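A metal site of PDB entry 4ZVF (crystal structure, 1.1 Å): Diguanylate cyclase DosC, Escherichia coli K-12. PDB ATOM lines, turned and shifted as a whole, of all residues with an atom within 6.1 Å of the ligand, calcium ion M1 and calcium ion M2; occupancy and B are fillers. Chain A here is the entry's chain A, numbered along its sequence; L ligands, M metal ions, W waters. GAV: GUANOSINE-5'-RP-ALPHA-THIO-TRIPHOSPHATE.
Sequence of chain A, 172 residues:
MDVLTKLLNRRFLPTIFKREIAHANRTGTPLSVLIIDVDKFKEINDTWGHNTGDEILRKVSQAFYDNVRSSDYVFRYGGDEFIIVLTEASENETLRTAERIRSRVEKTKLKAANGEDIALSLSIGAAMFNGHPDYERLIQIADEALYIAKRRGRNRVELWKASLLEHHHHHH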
ATOM      1  N   ASP A  37      22.142  -0.567  -6.414  1.00  0.00           N
ATOM      2  CA  ASP A  37      20.772  -0.813  -6.010  1.00  0.00           C
ATOM      3  C   ASP A  37      19.919   0.370  -6.451  1.00  0.00           C
ATOM      4  O   ASP A  37      20.186   1.522  -6.093  1.00  0.00           O
ATOM      5  CB  ASP A  37      20.764  -1.008  -4.491  1.00  0.00           C
ATOM      6  CG  ASP A  37      19.408  -1.316  -3.930  1.00  0.00           C
ATOM      7  OD1 ASP A  37      18.459  -0.585  -4.237  1.00  0.00           O
ATOM      8  OD2 ASP A  37      19.302  -2.257  -3.114  1.00  0.00           O
ATOM      9  N   VAL A  38      18.888   0.096  -7.256  1.00  0.00           N
ATOM     10  CA  VAL A  38      18.045   1.161  -7.790  1.00  0.00           C
ATOM     11  C   VAL A  38      17.297   1.862  -6.667  1.00  0.00           C
ATOM     12  O   VAL A  38      16.761   1.212  -5.759  1.00  0.00           O
ATOM     13  CB  VAL A  38      17.044   0.634  -8.846  1.00  0.00           C
ATOM     14  CG1 VAL A  38      16.175   1.774  -9.406  1.00  0.00           C
ATOM     15  CG2 VAL A  38      17.803  -0.089  -9.965  1.00  0.00           C
ATOM     16  N   ASP A  39      17.247   3.188  -6.721  1.00  0.00           N
ATOM     17  CA  ASP A  39      16.610   3.986  -5.680  1.00  0.00           C
ATOM     18  C   ASP A  39      15.099   4.004  -5.815  1.00  0.00           C
ATOM     19  O   ASP A  39      14.557   4.265  -6.905  1.00  0.00           O
ATOM     20  CB  ASP A  39      17.130   5.415  -5.735  1.00  0.00           C
ATOM     21  CG  ASP A  39      18.583   5.538  -5.299  1.00  0.00           C
ATOM     22  OD1 ASP A  39      19.066   4.696  -4.516  1.00  0.00           O
ATOM     23  OD2 ASP A  39      19.223   6.501  -5.749  1.00  0.00           O
ATOM     24  N   LYS A  40      14.411   3.700  -4.722  1.00  0.00           N
ATOM     25  CA  LYS A  40      12.939   3.871  -4.640  1.00  0.00           C
ATOM     26  C   LYS A  40      12.241   3.175  -5.817  1.00  0.00           C
ATOM     27  O   LYS A  40      11.318   3.712  -6.438  1.00  0.00           O
ATOM     28  CB  LYS A  40      12.557   5.355  -4.552  1.00  0.00           C
ATOM     29  CG  LYS A  40      13.145   6.038  -3.318  1.00  0.00           C
ATOM     30  CD  LYS A  40      12.597   7.449  -3.094  1.00  0.00           C
ATOM     31  CE  LYS A  40      13.191   8.101  -1.840  1.00  0.00           C
ATOM     32  NZ  LYS A  40      12.578   9.437  -1.567  1.00  0.00           N
ATOM     33  N   PHE A  41      12.708   1.968  -6.108  1.00  0.00           N
ATOM     34  CA  PHE A  41      12.176   1.196  -7.222  1.00  0.00           C
ATOM     35  C   PHE A  41      10.715   0.783  -6.988  1.00  0.00           C
ATOM     36  O   PHE A  41       9.943   0.643  -7.942  1.00  0.00           O
ATOM     37  CB  PHE A  41      13.067  -0.023  -7.475  1.00  0.00           C
ATOM     38  CG  PHE A  41      12.871  -0.663  -8.822  1.00  0.00           C
ATOM     39  CD1 PHE A  41      12.861   0.097  -9.983  1.00  0.00           C
ATOM     40  CD2 PHE A  41      12.740  -2.033  -8.921  1.00  0.00           C
ATOM     41  CE1 PHE A  41      12.698  -0.512 -11.225  1.00  0.00           C
ATOM     42  CE2 PHE A  41      12.594  -2.652 -10.163  1.00  0.00           C
ATOM     43  CZ  PHE A  41      12.567  -1.884 -11.301  1.00  0.00           C
ATOM     44  N   LYS A  42      10.321   0.596  -5.732  1.00  0.00           N
ATOM     45  CA  LYS A  42       8.918   0.319  -5.433  1.00  0.00           C
ATOM     46  C   LYS A  42       8.043   1.485  -5.889  1.00  0.00           C
ATOM     47  O   LYS A  42       6.993   1.286  -6.509  1.00  0.00           O
ATOM     48  CB  LYS A  42       8.699   0.023  -3.955  1.00  0.00           C
ATOM     49  CG  LYS A  42       7.243  -0.228  -3.588  1.00  0.00           C
ATOM     50  CD  LYS A  42       7.055  -0.491  -2.106  1.00  0.00           C
ATOM     51  CE  LYS A  42       7.564  -1.883  -1.729  1.00  0.00           C
ATOM     52  NZ  LYS A  42       6.967  -2.359  -0.446  1.00  0.00           N
ATOM     53  N   GLU A  43       8.486   2.705  -5.609  1.00  0.00           N
ATOM     54  CA  GLU A  43       7.763   3.890  -6.048  1.00  0.00           C
ATOM     55  C   GLU A  43       7.723   4.004  -7.565  1.00  0.00           C
ATOM     56  O   GLU A  43       6.699   4.404  -8.134  1.00  0.00           O
ATOM     57  CB  GLU A  43       8.374   5.163  -5.441  1.00  0.00           C
ATOM     58  CG  GLU A  43       8.159   5.309  -3.939  1.00  0.00           C
ATOM     59  CD  GLU A  43       8.622   6.648  -3.396  1.00  0.00           C
ATOM     60  OE1 GLU A  43       8.626   6.826  -2.155  1.00  0.00           O
ATOM     61  OE2 GLU A  43       8.987   7.536  -4.204  1.00  0.00           O
ATOM     62  N   ASN A  45       7.740   1.490  -9.725  1.00  0.00           N
ATOM     63  CA  ASN A  45       6.751   0.514 -10.176  1.00  0.00           C
ATOM     64  C   ASN A  45       5.320   0.922  -9.843  1.00  0.00           C
ATOM     65  O   ASN A  45       4.419   0.711 -10.638  1.00  0.00           O
ATOM     66  CB  ASN A  45       7.050  -0.869  -9.607  1.00  0.00           C
ATOM     67  CG  ASN A  45       8.219  -1.547 -10.303  1.00  0.00           C
ATOM     68  OD1 ASN A  45       8.087  -2.012 -11.427  1.00  0.00           O
ATOM     69  ND2 ASN A  45       9.354  -1.603  -9.641  1.00  0.00           N
ATOM     70  N   GLY A  49       4.242   1.706 -13.380  1.00  0.00           N
ATOM     71  CA  GLY A  49       3.919   0.341 -13.772  1.00  0.00           C
ATOM     72  C   GLY A  49       5.096  -0.616 -13.810  1.00  0.00           C
ATOM     73  O   GLY A  49       6.254  -0.212 -13.980  1.00  0.00           O
ATOM     74  N   HIS A  50       4.790  -1.905 -13.635  1.00  0.00           N
ATOM     75  CA  HIS A  50       5.794  -2.963 -13.611  1.00  0.00           C
ATOM     76  C   HIS A  50       6.575  -3.043 -14.936  1.00  0.00           C
ATOM     77  O   HIS A  50       7.781  -3.279 -14.927  1.00  0.00           O
ATOM     78  CB  HIS A  50       5.106  -4.297 -13.309  1.00  0.00           C
ATOM     79  CG  HIS A  50       6.046  -5.425 -12.967  1.00  0.00           C
ATOM     80  ND1 HIS A  50       6.658  -6.209 -13.926  1.00  0.00           N
ATOM     81  CD2 HIS A  50       6.452  -5.905 -11.773  1.00  0.00           C
ATOM     82  CE1 HIS A  50       7.412  -7.112 -13.333  1.00  0.00           C
ATOM     83  NE2 HIS A  50       7.313  -6.956 -12.027  1.00  0.00           N
ATOM     84  N   ASN A  51       5.883  -2.858 -16.059  1.00  0.00           N
ATOM     85  CA  ASN A  51       6.544  -2.865 -17.367  1.00  0.00           C
ATOM     86  C   ASN A  51       7.576  -1.747 -17.479  1.00  0.00           C
ATOM     87  O   ASN A  51       8.680  -1.951 -17.980  1.00  0.00           O
ATOM     88  CB  ASN A  51       5.534  -2.787 -18.528  1.00  0.00           C
ATOM     89  CG  ASN A  51       4.801  -4.109 -18.777  1.00  0.00           C
ATOM     90  OD1 ASN A  51       3.669  -4.305 -18.340  1.00  0.00           O
ATOM     91  ND2 ASN A  51       5.442  -5.016 -19.503  1.00  0.00           N
ATOM     92  N   THR A  52       7.211  -0.551 -17.003  1.00  0.00           N
ATOM     93  CA  THR A  52       8.172   0.558 -17.001  1.00  0.00           C
ATOM     94  C   THR A  52       9.378   0.215 -16.121  1.00  0.00           C
ATOM     95  O   THR A  52      10.545   0.469 -16.495  1.00  0.00           O
ATOM     96  CB  THR A  52       7.533   1.880 -16.545  1.00  0.00           C
ATOM     97  OG1 THR A  52       6.440   2.177 -17.419  1.00  0.00           O
ATOM     98  CG2 THR A  52       8.570   2.987 -16.627  1.00  0.00           C
ATOM     99  N   GLY A  53       9.113  -0.399 -14.970  1.00  0.00           N
ATOM    100  CA  GLY A  53      10.186  -0.851 -14.090  1.00  0.00           C
ATOM    101  C   GLY A  53      11.136  -1.805 -14.803  1.00  0.00           C
ATOM    102  O   GLY A  53      12.360  -1.679 -14.683  1.00  0.00           O
ATOM    103  N   ASP A  54      10.585  -2.726 -15.582  1.00  0.00           N
ATOM    104  CA  ASP A  54      11.395  -3.679 -16.332  1.00  0.00           C
ATOM    105  C   ASP A  54      12.239  -2.969 -17.403  1.00  0.00           C
ATOM    106  O   ASP A  54      13.386  -3.353 -17.639  1.00  0.00           O
ATOM    107  CB  ASP A  54      10.524  -4.761 -16.969  1.00  0.00           C
ATOM    108  CG  ASP A  54      10.077  -5.838 -15.969  1.00  0.00           C
ATOM    109  OD1 ASP A  54      10.349  -5.715 -14.765  1.00  0.00           O
ATOM    110  OD2 ASP A  54       9.422  -6.817 -16.413  1.00  0.00           O
ATOM    111  N   LEU A  57      15.181  -1.397 -15.671  1.00  0.00           N
ATOM    112  CA  LEU A  57      16.244  -2.369 -15.388  1.00  0.00           C
ATOM    113  C   LEU A  57      17.165  -2.572 -16.600  1.00  0.00           C
ATOM    114  O   LEU A  57      18.372  -2.716 -16.428  1.00  0.00           O
ATOM    115  CB  LEU A  57      15.665  -3.704 -14.906  1.00  0.00           C
ATOM    116  CG  LEU A  57      14.995  -3.655 -13.533  1.00  0.00           C
ATOM    117  CD1 LEU A  57      14.268  -4.959 -13.202  1.00  0.00           C
ATOM    118  CD2 LEU A  57      15.971  -3.274 -12.420  1.00  0.00           C
ATOM    119  N   ARG A  76      23.636  -9.876 -12.283  1.00  0.00           N
ATOM    120  CA  ARG A  76      22.348  -9.635 -11.673  1.00  0.00           C
ATOM    121  C   ARG A  76      22.358 -10.267 -10.283  1.00  0.00           C
ATOM    122  O   ARG A  76      22.536 -11.477 -10.157  1.00  0.00           O
ATOM    123  CB  ARG A  76      21.250 -10.299 -12.502  1.00  0.00           C
ATOM    124  CG  ARG A  76      19.834 -10.053 -12.006  1.00  0.00           C
ATOM    125  CD  ARG A  76      19.357  -8.649 -12.368  1.00  0.00           C
ATOM    126  NE  ARG A  76      17.983  -8.387 -11.933  1.00  0.00           N
ATOM    127  CZ  ARG A  76      16.903  -8.590 -12.680  1.00  0.00           C
ATOM    128  NH1 ARG A  76      17.026  -9.066 -13.914  1.00  0.00           N
ATOM    129  NH2 ARG A  76      15.691  -8.311 -12.192  1.00  0.00           N
ATOM    130  N   GLY A  78      20.014  -9.312  -7.526  1.00  0.00           N
ATOM    131  CA  GLY A  78      18.685  -9.378  -6.948  1.00  0.00           C
ATOM    132  C   GLY A  78      17.718  -8.702  -7.891  1.00  0.00           C
ATOM    133  O   GLY A  78      18.103  -8.319  -8.990  1.00  0.00           O
ATOM    134  N   GLY A  79      16.473  -8.517  -7.438  1.00  0.00           N
ATOM    135  CA  GLY A  79      15.443  -7.876  -8.254  1.00  0.00           C
ATOM    136  C   GLY A  79      15.887  -6.566  -8.879  1.00  0.00           C
ATOM    137  O   GLY A  79      15.703  -6.341 -10.075  1.00  0.00           O
ATOM    138  N   ASP A  80      16.480  -5.693  -8.067  1.00  0.00           N
ATOM    139  CA  ASP A  80      16.953  -4.400  -8.553  1.00  0.00           C
ATOM    140  C   ASP A  80      18.353  -4.113  -8.035  1.00  0.00           C
ATOM    141  O   ASP A  80      18.721  -2.959  -7.810  1.00  0.00           O
ATOM    142  CB  ASP A  80      15.986  -3.260  -8.177  1.00  0.00           C
ATOM    143  CG  ASP A  80      15.968  -2.953  -6.690  1.00  0.00           C
ATOM    144  OD1 ASP A  80      16.135  -3.882  -5.875  1.00  0.00           O
ATOM    145  OD2 ASP A  80      15.768  -1.766  -6.347  1.00  0.00           O
ATOM    146  N   GLU A  81      19.116  -5.195  -7.880  1.00  0.00           N
ATOM    147  CA  GLU A  81      20.469  -5.130  -7.351  1.00  0.00           C
ATOM    148  C   GLU A  81      21.439  -5.818  -8.291  1.00  0.00           C
ATOM    149  O   GLU A  81      21.114  -6.838  -8.909  1.00  0.00           O
ATOM    150  CB  GLU A  81      20.548  -5.801  -5.985  1.00  0.00           C
ATOM    151  CG  GLU A  81      19.878  -5.005  -4.873  1.00  0.00           C
ATOM    152  CD  GLU A  81      18.589  -5.631  -4.401  1.00  0.00           C
ATOM    153  OE1 GLU A  81      18.168  -6.659  -4.980  1.00  0.00           O
ATOM    154  OE2 GLU A  81      17.998  -5.088  -3.445  1.00  0.00           O
ATOM    155  N   LEU A 146      26.989   0.546   0.698  1.00  0.00           N
ATOM    156  CA  LEU A 146      25.729   0.789  -0.028  1.00  0.00           C
ATOM    157  C   LEU A 146      24.637   1.267   0.932  1.00  0.00           C
ATOM    158  O   LEU A 146      23.881   2.211   0.637  1.00  0.00           O
ATOM    159  CB  LEU A 146      25.278  -0.481  -0.741  1.00  0.00           C
ATOM    160  CG  LEU A 146      23.912  -0.404  -1.408  1.00  0.00           C
ATOM    161  CD1 LEU A 146      23.850   0.716  -2.455  1.00  0.00           C
ATOM    162  CD2 LEU A 146      23.555  -1.757  -2.024  1.00  0.00           C
ATOM    163  N   LYS A 150      22.543   4.826   0.890  1.00  0.00           N
ATOM    164  CA  LYS A 150      21.086   4.924   0.986  1.00  0.00           C
ATOM    165  C   LYS A 150      20.686   5.823   2.144  1.00  0.00           C
ATOM    166  O   LYS A 150      19.858   6.735   1.999  1.00  0.00           O
ATOM    167  CB  LYS A 150      20.457   3.538   1.173  1.00  0.00           C
ATOM    168  CG  LYS A 150      20.551   2.593  -0.023  1.00  0.00           C
ATOM    169  CD  LYS A 150      19.612   2.972  -1.171  1.00  0.00           C
ATOM    170  CE  LYS A 150      19.504   1.829  -2.177  1.00  0.00           C
ATOM    171  NZ  LYS A 150      18.643   2.164  -3.350  1.00  0.00           N
ATOM    172  N   ARG A 154      20.490   8.583  -0.787  1.00  0.00           N
ATOM    173  CA  ARG A 154      20.410   7.921  -2.104  1.00  0.00           C
ATOM    174  C   ARG A 154      21.021   8.790  -3.202  1.00  0.00           C
ATOM    175  O   ARG A 154      21.564   9.864  -2.937  1.00  0.00           O
ATOM    176  CB  ARG A 154      18.975   7.505  -2.444  1.00  0.00           C
ATOM    177  CG  ARG A 154      18.354   6.585  -1.421  1.00  0.00           C
ATOM    178  CD  ARG A 154      16.943   6.214  -1.847  1.00  0.00           C
ATOM    179  NE  ARG A 154      16.326   5.191  -0.993  1.00  0.00           N
ATOM    180  CZ  ARG A 154      15.640   5.445   0.112  1.00  0.00           C
ATOM    181  NH1 ARG A 154      15.097   4.438   0.798  1.00  0.00           N
ATOM    182  NH2 ARG A 154      15.491   6.693   0.558  1.00  0.00           N
HETATM  183  O6  GAV L   1      12.227  -7.930 -11.904  1.00  0.00           O
HETATM  184  C6  GAV L   1      11.629  -6.978 -11.398  1.00  0.00           C
HETATM  185  C5  GAV L   1      11.660  -6.746  -9.924  1.00  0.00           C
HETATM  186  C4  GAV L   1      11.004  -5.697  -9.372  1.00  0.00           C
HETATM  187  N3  GAV L   1      10.248  -4.784 -10.216  1.00  0.00           N
HETATM  188  C2  GAV L   1      10.216  -5.021 -11.623  1.00  0.00           C
HETATM  189  N2  GAV L   1       9.502  -4.155 -12.457  1.00  0.00           N
HETATM  190  N1  GAV L   1      10.911  -6.101 -12.204  1.00  0.00           N
HETATM  191  N7  GAV L   1      12.267  -7.426  -8.953  1.00  0.00           N
HETATM  192  C8  GAV L   1      11.996  -6.801  -7.786  1.00  0.00           C
HETATM  193  N9  GAV L   1      11.210  -5.754  -8.047  1.00  0.00           N
HETATM  194  C1' GAV L   1      10.579  -4.668  -7.353  1.00  0.00           C
HETATM  195  C2' GAV L   1       9.885  -5.232  -6.073  1.00  0.00           C
HETATM  196  O2' GAV L   1       8.592  -5.607  -6.341  1.00  0.00           O
HETATM  197  C3' GAV L   1       9.999  -4.098  -5.081  1.00  0.00           C
HETATM  198  O3' GAV L   1       8.701  -3.367  -5.020  1.00  0.00           O
HETATM  199  O4' GAV L   1      11.551  -3.984  -6.838  1.00  0.00           O
HETATM  200  C4' GAV L   1      10.966  -3.289  -5.534  1.00  0.00           C
HETATM  201  C5' GAV L   1      12.095  -3.074  -4.571  1.00  0.00           C
HETATM  202  O5' GAV L   1      11.539  -2.299  -3.508  1.00  0.00           O
HETATM  203  PA  GAV L   1      12.238  -2.211  -2.078  1.00  0.00           P
HETATM  204  S1A GAV L   1      13.395  -3.860  -1.682  1.00  0.00           S
HETATM  205  O2A GAV L   1      11.202  -2.038  -1.018  1.00  0.00           O
HETATM  206  O3A GAV L   1      13.208  -0.964  -2.106  1.00  0.00           O
HETATM  207  PB  GAV L   1      13.191   0.366  -3.007  1.00  0.00           P
HETATM  208  O1B GAV L   1      14.000   0.191  -4.258  1.00  0.00           O
HETATM  209  O2B GAV L   1      11.775   0.850  -3.233  1.00  0.00           O
HETATM  210  O3B GAV L   1      13.948   1.412  -2.038  1.00  0.00           O
HETATM  211  PG  GAV L   1      15.495   1.544  -1.699  1.00  0.00           P
HETATM  212  O1G GAV L   1      15.959   2.776  -2.464  1.00  0.00           O
HETATM  213  O3G GAV L   1      15.600   1.722  -0.210  1.00  0.00           O
HETATM  214  O2G GAV L   1      16.176   0.297  -2.220  1.00  0.00           O
HETATM  215 CA    CA M   1      16.170  -0.587  -4.408  1.00  0.00          CA
HETATM  216 CA    CA M   2      17.904  -3.611  -1.799  1.00  0.00          CA
HETATM  217  O   HOH W   1      17.003  -1.700  -0.726  1.00  0.00           O
HETATM  218  O   HOH W   2      10.628   0.551   0.079  1.00  0.00           O
HETATM  219  O   HOH W   3      10.192   2.989  -3.039  1.00  0.00           O
HETATM  220  O   HOH W   4      19.496  -1.770  -0.096  1.00  0.00           O
HETATM  221  O   HOH W   5      12.767 -10.305  -8.830  1.00  0.00           O
HETATM  222  O   HOH W   6      13.723  -9.080 -14.436  1.00  0.00           O
HETATM  223  O   HOH W   7      11.693  -2.401   2.185  1.00  0.00           O
HETATM  224  O   HOH W   8      16.038  -2.850  -3.418  1.00  0.00           O
HETATM  225  O   HOH W   9      16.673  -5.083  -0.359  1.00  0.00           O
HETATM  226  O   HOH W  10      17.613   0.980   1.331  1.00  0.00           O
HETATM  227  O   HOH W  11      19.816  -4.077  -0.512  1.00  0.00           O
HETATM  228  O   HOH W  12      10.589 -10.094 -13.150  1.00  0.00           O
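The side-chain carboxylate (OD1) of Asp 54 lies within hydrogen-bond range of a nitrogen (N1) of the ligand (2.7 Å).
N2 of the ligand lies within hydrogen-bond range of OD1 of Asn 45 (2.8 Å).
NE of Arg 154 is in salt-bridge range of O1G of the ligand, 2.9 Å away.
N of Phe 41 lies within hydrogen-bond range of O2B of the ligand.
O1G of the ligand is in hydrogen-bond range of N of Lys 40 (2.9 Å).
O1G of the ligand lies within salt-bridge range of NZ of Lys 150, 2.9 Å away.
The backbone NH (N) of Lys 42 is in hydrogen-bond range of an oxygen (O2B) of the ligand, 2.9 Å away.
O of His 50 lies within hydrogen-bond range of N2 of the ligand, at 3.1 Å.
O6 of the ligand sits at hydrogen-bond distance from NH2 of Arg 76 (3.5 Å).
O of Asp 37 is in hydrogen-bond range of NZ of Lys 150.
NZ of Lys 150 lies close to O of Val 38 (3.2 Å).
The backbone carbonyl oxygen (O) of Phe 41 lies within hydrogen-bond range of the side-chain amide nitrogen (ND2) of Asn 45 (2.9 Å).
NZ of Lys 150 is in salt-bridge range of OD1 of Asp 39 (2.8 Å).
The backbone carbonyl oxygen (O) of Gly 79 is in hydrogen-bond range of the guanidinium group (NH2) of Arg 76, 2.9 Å away.
The backbone carbonyl oxygen (O) of Gly 78 is in hydrogen-bond range of the guanidinium group (NE) of Arg 76, at 2.9 Å.
Residues that only touch the ligand: Gly 79 (3.3 Å), Asp 39 (3.5 Å), Leu 57 (3.7 Å) and Gly 53 (3.7 Å).
Hydrophobic or aromatic side chains that line the ligand: Phe 41, His 50 and Leu 57.
16 residues have an atom within 4 Å of the ligand: Asp 37, Val 38, Asp 39, Lys 40, Phe 41, Lys 42, Asn 45, His 50, Gly 53, Asp 54, Leu 57, Arg 76, Gly 79, Asp 80, Lys 150 and Arg 154.
The nearest printed residue that does not touch the ligand is Glu 43 (4.5 Å).
Merely in contact with calcium ion M1: Lys 150 (3.8 Å).
Within 4 Å of calcium ion M1: Asp 37, Val 38, Asp 80 and Lys 150.
Two residues have an atom within 4 Å of calcium ion M2: Asp 37 and Glu 81.
The nearest printed residue that does not touch calcium ion M2 is Asp 80 (4.5 Å).
Calcium ion M1 is bound by the side-chain carboxylate of Asp 37 (2.3 Å), the side-chain carboxylate of Asp 80 (2.3 Å), an oxygen (O1B) of the ligand (2.3 Å), the backbone carbonyl oxygen of Val 38 (2.3 Å), an oxygen (O2G) of the ligand (2.4 Å) and water W8 (2.5 Å).
Calcium ion M2 is bound by OE2 of Glu 81 (2.2 Å), OD2 of Asp 37 (2.3 Å), water W11 (2.4 Å), water W1 (2.4 Å), water W9 (2.4 Å) and water W8 (2.6 Å).
Calcium ion M2 has six donor atoms within binding distance.
Slightly farther from calcium ion M2 lies water W4 (3.0 Å).
Water W8 lies within hydrogen-bond range of OD1 of Asp 80 (2.7 Å) and S1A of the ligand (3.3 Å).
Water W3 bridges an oxygen (O2B) of the ligand (2.7 Å) and the backbone NH of Glu 43 (3.1 Å).
Water W6 lies within hydrogen-bond range of the guanidinium group of Arg 76 and an oxygen (O6) of the ligand.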
